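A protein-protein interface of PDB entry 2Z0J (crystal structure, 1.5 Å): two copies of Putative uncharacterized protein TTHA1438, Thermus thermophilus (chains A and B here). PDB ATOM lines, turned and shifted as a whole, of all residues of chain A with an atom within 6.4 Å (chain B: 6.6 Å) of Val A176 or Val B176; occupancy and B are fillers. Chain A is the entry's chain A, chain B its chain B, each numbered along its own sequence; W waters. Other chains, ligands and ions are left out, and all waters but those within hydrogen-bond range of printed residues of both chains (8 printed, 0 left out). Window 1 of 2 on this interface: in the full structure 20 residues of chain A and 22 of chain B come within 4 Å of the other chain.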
ATOM      1  N   VAL A   7     -13.473  -1.938  -3.671  1.00  0.00           N
ATOM      2  CA  VAL A   7     -13.704  -1.380  -2.331  1.00  0.00           C
ATOM      3  C   VAL A   7     -13.352   0.076  -2.190  1.00  0.00           C
ATOM      4  O   VAL A   7     -13.803   0.717  -1.231  1.00  0.00           O
ATOM      5  CB  VAL A   7     -12.962  -2.198  -1.236  1.00  0.00           C
ATOM      6  CG1 VAL A   7     -13.329  -3.663  -1.355  1.00  0.00           C
ATOM      7  CG2 VAL A   7     -11.480  -1.965  -1.365  1.00  0.00           C
ATOM      8  N   ALA A 147     -11.246   2.313   2.556  1.00  0.00           N
ATOM      9  CA  ALA A 147     -12.604   1.776   2.406  1.00  0.00           C
ATOM     10  C   ALA A 147     -13.544   2.132   3.537  1.00  0.00           C
ATOM     11  O   ALA A 147     -13.131   2.270   4.685  1.00  0.00           O
ATOM     12  CB  ALA A 147     -12.514   0.259   2.232  1.00  0.00           C
ATOM     13  N   GLY A 148     -14.818   2.303   3.202  1.00  0.00           N
ATOM     14  CA  GLY A 148     -15.838   2.617   4.201  1.00  0.00           C
ATOM     15  C   GLY A 148     -16.697   1.406   4.489  1.00  0.00           C
ATOM     16  O   GLY A 148     -17.130   0.684   3.583  1.00  0.00           O
ATOM     17  N   LEU A 149     -16.894   1.134   5.768  1.00  0.00           N
ATOM     18  CA  LEU A 149     -17.715  -0.013   6.227  1.00  0.00           C
ATOM     19  C   LEU A 149     -19.148   0.139   5.716  1.00  0.00           C
ATOM     20  O   LEU A 149     -19.796  -0.850   5.346  1.00  0.00           O
ATOM     21  CB  LEU A 149     -17.730  -0.039   7.767  1.00  0.00           C
ATOM     22  CG  LEU A 149     -18.589  -1.107   8.423  1.00  0.00           C
ATOM     23  CD1 LEU A 149     -17.931  -2.444   8.173  1.00  0.00           C
ATOM     24  CD2 LEU A 149     -18.698  -0.812   9.931  1.00  0.00           C
ATOM     25  N   LEU A 152     -19.244  -0.600   1.880  1.00  0.00           N
ATOM     26  CA  LEU A 152     -19.109  -2.060   1.656  1.00  0.00           C
ATOM     27  C   LEU A 152     -20.352  -2.832   2.142  1.00  0.00           C
ATOM     28  O   LEU A 152     -20.742  -3.772   1.462  1.00  0.00           O
ATOM     29  CB  LEU A 152     -17.828  -2.594   2.353  1.00  0.00           C
ATOM     30  CG  LEU A 152     -16.602  -2.433   1.443  1.00  0.00           C
ATOM     31  CD1 LEU A 152     -15.350  -2.837   2.200  1.00  0.00           C
ATOM     32  CD2 LEU A 152     -16.661  -3.420   0.273  1.00  0.00           C
ATOM     33  N   GLU A 171     -15.911 -11.915  -7.482  1.00  0.00           N
ATOM     34  CA  GLU A 171     -14.481 -11.856  -7.282  1.00  0.00           C
ATOM     35  C   GLU A 171     -14.174 -11.425  -5.828  1.00  0.00           C
ATOM     36  O   GLU A 171     -15.078 -11.449  -4.990  1.00  0.00           O
ATOM     37  CB  GLU A 171     -13.780 -11.015  -8.375  1.00  0.00           C
ATOM     38  CG  GLU A 171     -14.244  -9.567  -8.632  1.00  0.00           C
ATOM     39  CD  GLU A 171     -14.094  -8.721  -7.367  1.00  0.00           C
ATOM     40  OE1 GLU A 171     -15.134  -8.580  -6.719  1.00  0.00           O
ATOM     41  OE2 GLU A 171     -12.970  -8.229  -7.053  1.00  0.00           O
ATOM     42  N   ASP A 172     -12.932 -11.103  -5.523  1.00  0.00           N
ATOM     43  CA  ASP A 172     -12.552 -10.879  -4.121  1.00  0.00           C
ATOM     44  C   ASP A 172     -13.368  -9.774  -3.452  1.00  0.00           C
ATOM     45  O   ASP A 172     -13.853  -9.921  -2.297  1.00  0.00           O
ATOM     46  CB  ASP A 172     -11.056 -10.481  -4.037  1.00  0.00           C
ATOM     47  CG  ASP A 172     -10.080 -11.635  -4.224  1.00  0.00           C
ATOM     48  OD1 ASP A 172     -10.405 -12.566  -4.939  1.00  0.00           O
ATOM     49  OD2 ASP A 172      -8.960 -11.529  -3.648  1.00  0.00           O
ATOM     50  N   GLY A 173     -13.484  -8.637  -4.106  1.00  0.00           N
ATOM     51  CA  GLY A 173     -14.241  -7.551  -3.492  1.00  0.00           C
ATOM     52  C   GLY A 173     -15.674  -7.900  -3.207  1.00  0.00           C
ATOM     53  O   GLY A 173     -16.205  -7.505  -2.183  1.00  0.00           O
ATOM     54  N   ALA A 174     -16.302  -8.625  -4.112  1.00  0.00           N
ATOM     55  CA  ALA A 174     -17.684  -9.014  -3.906  1.00  0.00           C
ATOM     56  C   ALA A 174     -17.789  -9.963  -2.699  1.00  0.00           C
ATOM     57  O   ALA A 174     -18.793  -9.898  -1.942  1.00  0.00           O
ATOM     58  CB  ALA A 174     -18.197  -9.661  -5.174  1.00  0.00           C
ATOM     59  N   ARG A 175     -16.810 -10.872  -2.520  1.00  0.00           N
ATOM     60  CA  ARG A 175     -16.891 -11.766  -1.337  1.00  0.00           C
ATOM     61  C   ARG A 175     -16.671 -10.955  -0.060  1.00  0.00           C
ATOM     62  O   ARG A 175     -17.277 -11.237   0.966  1.00  0.00           O
ATOM     63  CB  ARG A 175     -15.848 -12.908  -1.462  1.00  0.00           C
ATOM     64  CG  ARG A 175     -16.217 -13.882  -2.613  1.00  0.00           C
ATOM     65  CD  ARG A 175     -15.362 -15.139  -2.487  1.00  0.00           C
ATOM     66  NE  ARG A 175     -15.478 -15.971  -3.680  1.00  0.00           N
ATOM     67  CZ  ARG A 175     -16.435 -16.843  -3.916  1.00  0.00           C
ATOM     68  NH1 ARG A 175     -17.408 -17.057  -3.042  1.00  0.00           N
ATOM     69  NH2 ARG A 175     -16.433 -17.479  -5.095  1.00  0.00           N
ATOM     70  N   VAL A 176     -15.809  -9.933  -0.101  1.00  0.00           N
ATOM     71  CA  VAL A 176     -15.619  -9.062   1.069  1.00  0.00           C
ATOM     72  C   VAL A 176     -16.955  -8.327   1.374  1.00  0.00           C
ATOM     73  O   VAL A 176     -17.403  -8.245   2.510  1.00  0.00           O
ATOM     74  CB  VAL A 176     -14.520  -8.048   0.755  1.00  0.00           C
ATOM     75  CG1 VAL A 176     -14.464  -6.921   1.859  1.00  0.00           C
ATOM     76  CG2 VAL A 176     -13.143  -8.774   0.667  1.00  0.00           C
ATOM     77  N   ALA A 177     -17.611  -7.778   0.338  1.00  0.00           N
ATOM     78  CA  ALA A 177     -18.864  -7.038   0.562  1.00  0.00           C
ATOM     79  C   ALA A 177     -19.925  -7.948   1.156  1.00  0.00           C
ATOM     80  O   ALA A 177     -20.641  -7.554   2.091  1.00  0.00           O
ATOM     81  CB  ALA A 177     -19.327  -6.423  -0.761  1.00  0.00           C
ATOM     82  N   LEU A 178     -20.036  -9.164   0.617  1.00  0.00           N
ATOM     83  CA  LEU A 178     -21.050 -10.092   1.166  1.00  0.00           C
ATOM     84  C   LEU A 178     -20.689 -10.465   2.595  1.00  0.00           C
ATOM     85  O   LEU A 178     -21.586 -10.621   3.422  1.00  0.00           O
ATOM     86  CB  LEU A 178     -21.108 -11.337   0.279  1.00  0.00           C
ATOM     87  CG  LEU A 178     -21.788 -11.126  -1.057  1.00  0.00           C
ATOM     88  CD1 LEU A 178     -21.472 -12.336  -1.945  1.00  0.00           C
ATOM     89  CD2 LEU A 178     -23.298 -11.018  -0.839  1.00  0.00           C
ATOM     90  N   ALA A 179     -19.400 -10.569   2.921  1.00  0.00           N
ATOM     91  CA  ALA A 179     -19.045 -10.887   4.307  1.00  0.00           C
ATOM     92  C   ALA A 179     -19.484  -9.744   5.250  1.00  0.00           C
ATOM     93  O   ALA A 179     -19.913  -9.970   6.364  1.00  0.00           O
ATOM     94  CB  ALA A 179     -17.473 -11.123   4.418  1.00  0.00           C
ATOM     95  N   VAL A 180     -19.283  -8.497   4.822  1.00  0.00           N
ATOM     96  CA  VAL A 180     -19.701  -7.360   5.650  1.00  0.00           C
ATOM     97  C   VAL A 180     -21.217  -7.383   5.837  1.00  0.00           C
ATOM     98  O   VAL A 180     -21.715  -7.156   6.925  1.00  0.00           O
ATOM     99  CB  VAL A 180     -19.224  -6.026   4.983  1.00  0.00           C
ATOM    100  CG1 VAL A 180     -19.749  -4.798   5.777  1.00  0.00           C
ATOM    101  CG2 VAL A 180     -17.677  -5.999   4.924  1.00  0.00           C
ATOM    102  N   LYS A 181     -21.961  -7.662   4.769  1.00  0.00           N
ATOM    103  CA  LYS A 181     -23.424  -7.732   4.905  1.00  0.00           C
ATOM    104  C   LYS A 181     -23.778  -8.809   5.935  1.00  0.00           C
ATOM    105  O   LYS A 181     -24.614  -8.574   6.817  1.00  0.00           O
ATOM    106  CB  LYS A 181     -24.053  -8.089   3.534  1.00  0.00           C
ATOM    107  CG  LYS A 181     -25.570  -8.482   3.554  1.00  0.00           C
ATOM    108  CD  LYS A 181     -26.458  -7.547   4.255  1.00  0.00           C
ATOM    109  CE  LYS A 181     -27.939  -7.964   3.931  1.00  0.00           C
ATOM    110  NZ  LYS A 181     -28.275  -9.373   4.397  1.00  0.00           N
ATOM    111  N   TYR A 184     -23.570  -7.884   9.720  1.00  0.00           N
ATOM    112  CA  TYR A 184     -24.485  -6.895  10.307  1.00  0.00           C
ATOM    113  C   TYR A 184     -25.920  -7.067   9.868  1.00  0.00           C
ATOM    114  O   TYR A 184     -26.324  -6.505   8.878  1.00  0.00           O
ATOM    115  CB  TYR A 184     -24.040  -5.472   9.917  1.00  0.00           C
ATOM    116  CG  TYR A 184     -22.675  -5.146  10.464  1.00  0.00           C
ATOM    117  CD1 TYR A 184     -22.526  -4.767  11.781  1.00  0.00           C
ATOM    118  CD2 TYR A 184     -21.520  -5.292   9.662  1.00  0.00           C
ATOM    119  CE1 TYR A 184     -21.254  -4.547  12.344  1.00  0.00           C
ATOM    120  CE2 TYR A 184     -20.243  -5.069  10.210  1.00  0.00           C
ATOM    121  CZ  TYR A 184     -20.133  -4.699  11.550  1.00  0.00           C
ATOM    122  OH  TYR A 184     -18.864  -4.496  12.046  1.00  0.00           O
ATOM    123  N   VAL B   7      -7.178  -1.492   3.593  1.00  0.00           N
ATOM    124  CA  VAL B   7      -7.436  -2.608   2.685  1.00  0.00           C
ATOM    125  C   VAL B   7      -6.612  -2.637   1.434  1.00  0.00           C
ATOM    126  O   VAL B   7      -6.512  -3.693   0.798  1.00  0.00           O
ATOM    127  CB  VAL B   7      -8.929  -2.694   2.292  1.00  0.00           C
ATOM    128  CG1 VAL B   7      -9.787  -2.625   3.536  1.00  0.00           C
ATOM    129  CG2 VAL B   7      -9.268  -1.636   1.292  1.00  0.00           C
ATOM    130  N   ALA B 147      -8.562  -4.688  -3.525  1.00  0.00           N
ATOM    131  CA  ALA B 147      -8.271  -5.449  -2.319  1.00  0.00           C
ATOM    132  C   ALA B 147      -8.285  -6.937  -2.523  1.00  0.00           C
ATOM    133  O   ALA B 147      -9.013  -7.424  -3.336  1.00  0.00           O
ATOM    134  CB  ALA B 147      -9.282  -5.059  -1.245  1.00  0.00           C
ATOM    135  N   GLY B 148      -7.463  -7.631  -1.739  1.00  0.00           N
ATOM    136  CA  GLY B 148      -7.471  -9.077  -1.857  1.00  0.00           C
ATOM    137  C   GLY B 148      -8.217  -9.717  -0.686  1.00  0.00           C
ATOM    138  O   GLY B 148      -7.983  -9.342   0.467  1.00  0.00           O
ATOM    139  N   LEU B 149      -9.051 -10.694  -0.988  1.00  0.00           N
ATOM    140  CA  LEU B 149      -9.802 -11.437   0.019  1.00  0.00           C
ATOM    141  C   LEU B 149      -8.826 -12.150   0.974  1.00  0.00           C
ATOM    142  O   LEU B 149      -9.065 -12.184   2.178  1.00  0.00           O
ATOM    143  CB  LEU B 149     -10.661 -12.459  -0.701  1.00  0.00           C
ATOM    144  CG  LEU B 149     -11.404 -13.430   0.232  1.00  0.00           C
ATOM    145  CD1 LEU B 149     -12.416 -12.719   1.090  1.00  0.00           C
ATOM    146  CD2 LEU B 149     -12.086 -14.495  -0.635  1.00  0.00           C
ATOM    147  N   LEU B 152      -7.145  -9.529   3.292  1.00  0.00           N
ATOM    148  CA  LEU B 152      -8.109  -9.032   4.279  1.00  0.00           C
ATOM    149  C   LEU B 152      -8.460 -10.102   5.300  1.00  0.00           C
ATOM    150  O   LEU B 152      -8.656  -9.794   6.453  1.00  0.00           O
ATOM    151  CB  LEU B 152      -9.365  -8.493   3.561  1.00  0.00           C
ATOM    152  CG  LEU B 152      -9.259  -7.010   3.245  1.00  0.00           C
ATOM    153  CD1 LEU B 152     -10.484  -6.667   2.346  1.00  0.00           C
ATOM    154  CD2 LEU B 152      -9.281  -6.206   4.532  1.00  0.00           C
ATOM    155  N   GLY B 156      -7.995  -9.862   9.268  1.00  0.00           N
ATOM    156  CA  GLY B 156      -9.030 -10.207  10.224  1.00  0.00           C
ATOM    157  C   GLY B 156      -8.498 -11.161  11.297  1.00  0.00           C
ATOM    158  O   GLY B 156      -8.852 -11.002  12.469  1.00  0.00           O
ATOM    159  N   GLU B 171     -11.302   0.765  13.562  1.00  0.00           N
ATOM    160  CA  GLU B 171     -11.953   1.682  12.611  1.00  0.00           C
ATOM    161  C   GLU B 171     -12.568   0.846  11.477  1.00  0.00           C
ATOM    162  O   GLU B 171     -12.707  -0.371  11.615  1.00  0.00           O
ATOM    163  CB  GLU B 171     -11.017   2.805  12.138  1.00  0.00           C
ATOM    164  CG  GLU B 171      -9.628   2.417  11.534  1.00  0.00           C
ATOM    165  CD  GLU B 171      -9.748   1.515  10.319  1.00  0.00           C
ATOM    166  OE1 GLU B 171     -10.050   2.024   9.217  1.00  0.00           O
ATOM    167  OE2 GLU B 171      -9.595   0.308  10.492  1.00  0.00           O
ATOM    168  N   ASP B 172     -12.968   1.474  10.379  1.00  0.00           N
ATOM    169  CA  ASP B 172     -13.711   0.731   9.355  1.00  0.00           C
ATOM    170  C   ASP B 172     -12.993  -0.444   8.766  1.00  0.00           C
ATOM    171  O   ASP B 172     -13.592  -1.509   8.599  1.00  0.00           O
ATOM    172  CB  ASP B 172     -14.108   1.659   8.209  1.00  0.00           C
ATOM    173  CG  ASP B 172     -15.220   2.650   8.577  1.00  0.00           C
ATOM    174  OD1 ASP B 172     -15.378   3.011   9.760  1.00  0.00           O
ATOM    175  OD2 ASP B 172     -15.929   3.073   7.625  1.00  0.00           O
ATOM    176  N   GLY B 173     -11.736  -0.250   8.394  1.00  0.00           N
ATOM    177  CA  GLY B 173     -11.049  -1.340   7.764  1.00  0.00           C
ATOM    178  C   GLY B 173     -10.954  -2.538   8.659  1.00  0.00           C
ATOM    179  O   GLY B 173     -11.063  -3.684   8.198  1.00  0.00           O
ATOM    180  N   ALA B 174     -10.721  -2.275   9.933  1.00  0.00           N
ATOM    181  CA  ALA B 174     -10.621  -3.385  10.867  1.00  0.00           C
ATOM    182  C   ALA B 174     -11.963  -4.119  11.034  1.00  0.00           C
ATOM    183  O   ALA B 174     -11.962  -5.344  11.111  1.00  0.00           O
ATOM    184  CB  ALA B 174     -10.125  -2.856  12.223  1.00  0.00           C
ATOM    185  N   ARG B 175     -13.080  -3.375  11.039  1.00  0.00           N
ATOM    186  CA  ARG B 175     -14.399  -4.026  11.118  1.00  0.00           C
ATOM    187  C   ARG B 175     -14.632  -4.839   9.821  1.00  0.00           C
ATOM    188  O   ARG B 175     -15.221  -5.911   9.868  1.00  0.00           O
ATOM    189  CB  ARG B 175     -15.510  -2.983  11.326  1.00  0.00           C
ATOM    190  CG  ARG B 175     -15.410  -2.408  12.741  1.00  0.00           C
ATOM    191  CD  ARG B 175     -16.610  -1.470  13.074  1.00  0.00           C
ATOM    192  NE  ARG B 175     -16.342  -0.521  14.165  1.00  0.00           N
ATOM    193  CZ  ARG B 175     -16.493  -0.816  15.443  1.00  0.00           C
ATOM    194  NH1 ARG B 175     -16.903  -2.027  15.796  1.00  0.00           N
ATOM    195  NH2 ARG B 175     -16.257   0.107  16.370  1.00  0.00           N
ATOM    196  N   VAL B 176     -14.183  -4.340   8.667  1.00  0.00           N
ATOM    197  CA  VAL B 176     -14.319  -5.099   7.448  1.00  0.00           C
ATOM    198  C   VAL B 176     -13.504  -6.370   7.529  1.00  0.00           C
ATOM    199  O   VAL B 176     -13.988  -7.475   7.146  1.00  0.00           O
ATOM    200  CB  VAL B 176     -13.905  -4.258   6.205  1.00  0.00           C
ATOM    201  CG1 VAL B 176     -13.804  -5.184   4.986  1.00  0.00           C
ATOM    202  CG2 VAL B 176     -14.914  -3.131   5.944  1.00  0.00           C
ATOM    203  N   ALA B 177     -12.232  -6.236   7.986  1.00  0.00           N
ATOM    204  CA  ALA B 177     -11.390  -7.432   8.108  1.00  0.00           C
ATOM    205  C   ALA B 177     -11.951  -8.510   9.063  1.00  0.00           C
ATOM    206  O   ALA B 177     -11.938  -9.687   8.744  1.00  0.00           O
ATOM    207  CB  ALA B 177      -9.954  -7.012   8.533  1.00  0.00           C
ATOM    208  N   LEU B 178     -12.523  -8.053  10.164  1.00  0.00           N
ATOM    209  CA  LEU B 178     -13.155  -8.977  11.133  1.00  0.00           C
ATOM    210  C   LEU B 178     -14.356  -9.623  10.485  1.00  0.00           C
ATOM    211  O   LEU B 178     -14.594 -10.802  10.708  1.00  0.00           O
ATOM    212  CB  LEU B 178     -13.540  -8.222  12.403  1.00  0.00           C
ATOM    213  CG  LEU B 178     -12.319  -7.809  13.246  1.00  0.00           C
ATOM    214  CD1 LEU B 178     -12.740  -6.786  14.360  1.00  0.00           C
ATOM    215  CD2 LEU B 178     -11.643  -9.054  13.896  1.00  0.00           C
ATOM    216  N   ALA B 179     -15.113  -8.882   9.667  1.00  0.00           N
ATOM    217  CA  ALA B 179     -16.274  -9.491   8.997  1.00  0.00           C
ATOM    218  C   ALA B 179     -15.813 -10.597   8.014  1.00  0.00           C
ATOM    219  O   ALA B 179     -16.465 -11.639   7.870  1.00  0.00           O
ATOM    220  CB  ALA B 179     -17.053  -8.376   8.246  1.00  0.00           C
ATOM    221  N   VAL B 180     -14.690 -10.356   7.312  1.00  0.00           N
ATOM    222  CA  VAL B 180     -14.157 -11.368   6.384  1.00  0.00           C
ATOM    223  C   VAL B 180     -13.732 -12.625   7.165  1.00  0.00           C
ATOM    224  O   VAL B 180     -14.030 -13.751   6.737  1.00  0.00           O
ATOM    225  CB  VAL B 180     -12.971 -10.803   5.572  1.00  0.00           C
ATOM    226  CG1 VAL B 180     -12.319 -11.934   4.735  1.00  0.00           C
ATOM    227  CG2 VAL B 180     -13.512  -9.703   4.593  1.00  0.00           C
ATOM    228  N   LYS B 181     -13.029 -12.413   8.279  1.00  0.00           N
ATOM    229  CA  LYS B 181     -12.664 -13.563   9.144  1.00  0.00           C
ATOM    230  C   LYS B 181     -13.907 -14.312   9.613  1.00  0.00           C
ATOM    231  O   LYS B 181     -13.945 -15.537   9.500  1.00  0.00           O
ATOM    232  CB  LYS B 181     -11.854 -13.067  10.362  1.00  0.00           C
ATOM    233  CG  LYS B 181     -11.662 -14.091  11.549  1.00  0.00           C
ATOM    234  CD  LYS B 181     -10.946 -15.271  11.053  1.00  0.00           C
ATOM    235  CE  LYS B 181     -10.498 -16.178  12.231  1.00  0.00           C
ATOM    236  NZ  LYS B 181     -11.611 -16.542  13.168  1.00  0.00           N
ATOM    237  N   TYR B 184     -15.425 -16.619   6.917  1.00  0.00           N
ATOM    238  CA  TYR B 184     -14.616 -17.788   6.573  1.00  0.00           C
ATOM    239  C   TYR B 184     -13.884 -18.397   7.826  1.00  0.00           C
ATOM    240  O   TYR B 184     -12.704 -18.139   8.122  1.00  0.00           O
ATOM    241  CB  TYR B 184     -13.659 -17.417   5.447  1.00  0.00           C
ATOM    242  CG  TYR B 184     -14.394 -16.959   4.230  1.00  0.00           C
ATOM    243  CD1 TYR B 184     -15.008 -17.873   3.376  1.00  0.00           C
ATOM    244  CD2 TYR B 184     -14.544 -15.587   3.953  1.00  0.00           C
ATOM    245  CE1 TYR B 184     -15.744 -17.461   2.279  1.00  0.00           C
ATOM    246  CE2 TYR B 184     -15.277 -15.158   2.878  1.00  0.00           C
ATOM    247  CZ  TYR B 184     -15.883 -16.105   2.019  1.00  0.00           C
ATOM    248  OH  TYR B 184     -16.557 -15.772   0.877  1.00  0.00           O
HETATM  249  O   HOH W   1     -18.300  -4.352  14.597  1.00  0.00           O
HETATM  250  O   HOH W   2     -16.955  -6.574  11.836  1.00  0.00           O
HETATM  251  O   HOH W   3      -8.816   0.936   3.726  1.00  0.00           O
HETATM  252  O   HOH W   4     -11.485   3.408   6.503  1.00  0.00           O
HETATM  253  O   HOH W   5     -11.140  -3.533  -4.447  1.00  0.00           O
HETATM  254  O   HOH W   6     -19.206 -11.933   8.151  1.00  0.00           O
HETATM  255  O   HOH W   7     -18.405 -13.758   1.262  1.00  0.00           O
HETATM  256  O   HOH W   8      -9.864  -7.628  -5.924  1.00  0.00           O
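N of Leu A149 is in hydrogen-bond range of OD2 of Asp B172 (2.9 Å). The backbone NH of Leu B149 lies within hydrogen-bond range of the side-chain carboxylate of Asp A172.
Val A7 touches Ala B147 (CG2 to CB, 3.8 Å). CB of Asp B172 touches O of Ala A147 (3.7 Å). CA of Gly A148 touches OD2 of Asp B172, 3.5 Å away. CD2 of Leu A149 touches CD of Arg B175, 3.8 Å away. CD1 of Leu A149 touches CG2 of Val B176 (3.8 Å). OD2 of Asp A172 touches CA of Gly B148, 3.4 Å away. Ala A179 touches Val B180. Val A180 touches Val B176 (CG2 to CG1, 3.96 Å). CB of Ala B179 touches CA of Val A180, 3.8 Å away. Tyr A184 touches Arg B175 (OH to CB, 3.7 Å).
Of the printed residues of chain B, Val A176 touches Leu B152 (3.8 Å) and Val B176 (3.6 Å). Printed residues of chain A within 4 Å of Val B176: Leu A149, Leu A152, Val A176 and Val A180. Printed residues of chain B within 4 Å of Leu A152: Val B176. Printed residues of chain B within 4 Å of Ala A147: Val B7 and Asp B172. Printed residues of chain A within 4 Å of Tyr B184: Arg A175 (3.6 Å). Glu B171 touches none of the printed residues of chain A.
Of the 17 printed residues of chain A, 11 touch a printed residue of chain B. Hydrophobic or aromatic side chains of chain A within 4 Å of the printed part of chain B: Val A7, Ala A147, Leu A149, Leu A152, Val A176, Ala A179, Val A180 and Tyr A184. Of the 18 printed residues of chain B, 11 touch a printed residue of chain A. Hydrophobic or aromatic side chains of chain B that line the printed part of chain A: Val B7, Ala B147, Leu B149, Leu B152, Val B176, Ala B179 and Tyr B184. Among the printed residues, no Asp or Glu carboxylate lies within 4 Å of a Lys or Arg side-chain nitrogen of the other chain.
Val A7 touches Ala B147, and with the chains exchanged Ala A147 touches Val B7. Ala A147 touches Asp B172, and with the chains exchanged Asp A172 touches Ala B147. Leu A149 touches Asp B172, and with the chains exchanged Asp A172 touches Leu B149. Val A180 touches Val B176, but with the chains exchanged Val A176 does not touch Val B180 (4.02 Å). Of the 21 pairs that touch across the chains among the printed residues, 19 have their exchanged pair printed and touching as well.
Water W1 lies within hydrogen-bond range of OH of Tyr A184 and NH1 of Arg B175. Water W4 lies within hydrogen-bond range of the backbone carbonyl oxygen (O) of Ala A147 and the side-chain carboxylate (OE1) of Glu B171. Water W8 bridges O of Ala B147 and OE2 of Glu A171. Water W6 lies within hydrogen-bond range of the backbone carbonyl oxygen of Ala A179 (2.7 Å) and the backbone carbonyl oxygen of Ala B179 (2.8 Å). Water W7 bridges the side-chain hydroxyl of Tyr B184 and the backbone carbonyl oxygen of Arg A175. Water W3 lies within hydrogen-bond range of N of Val B7 and N of Ala A147.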
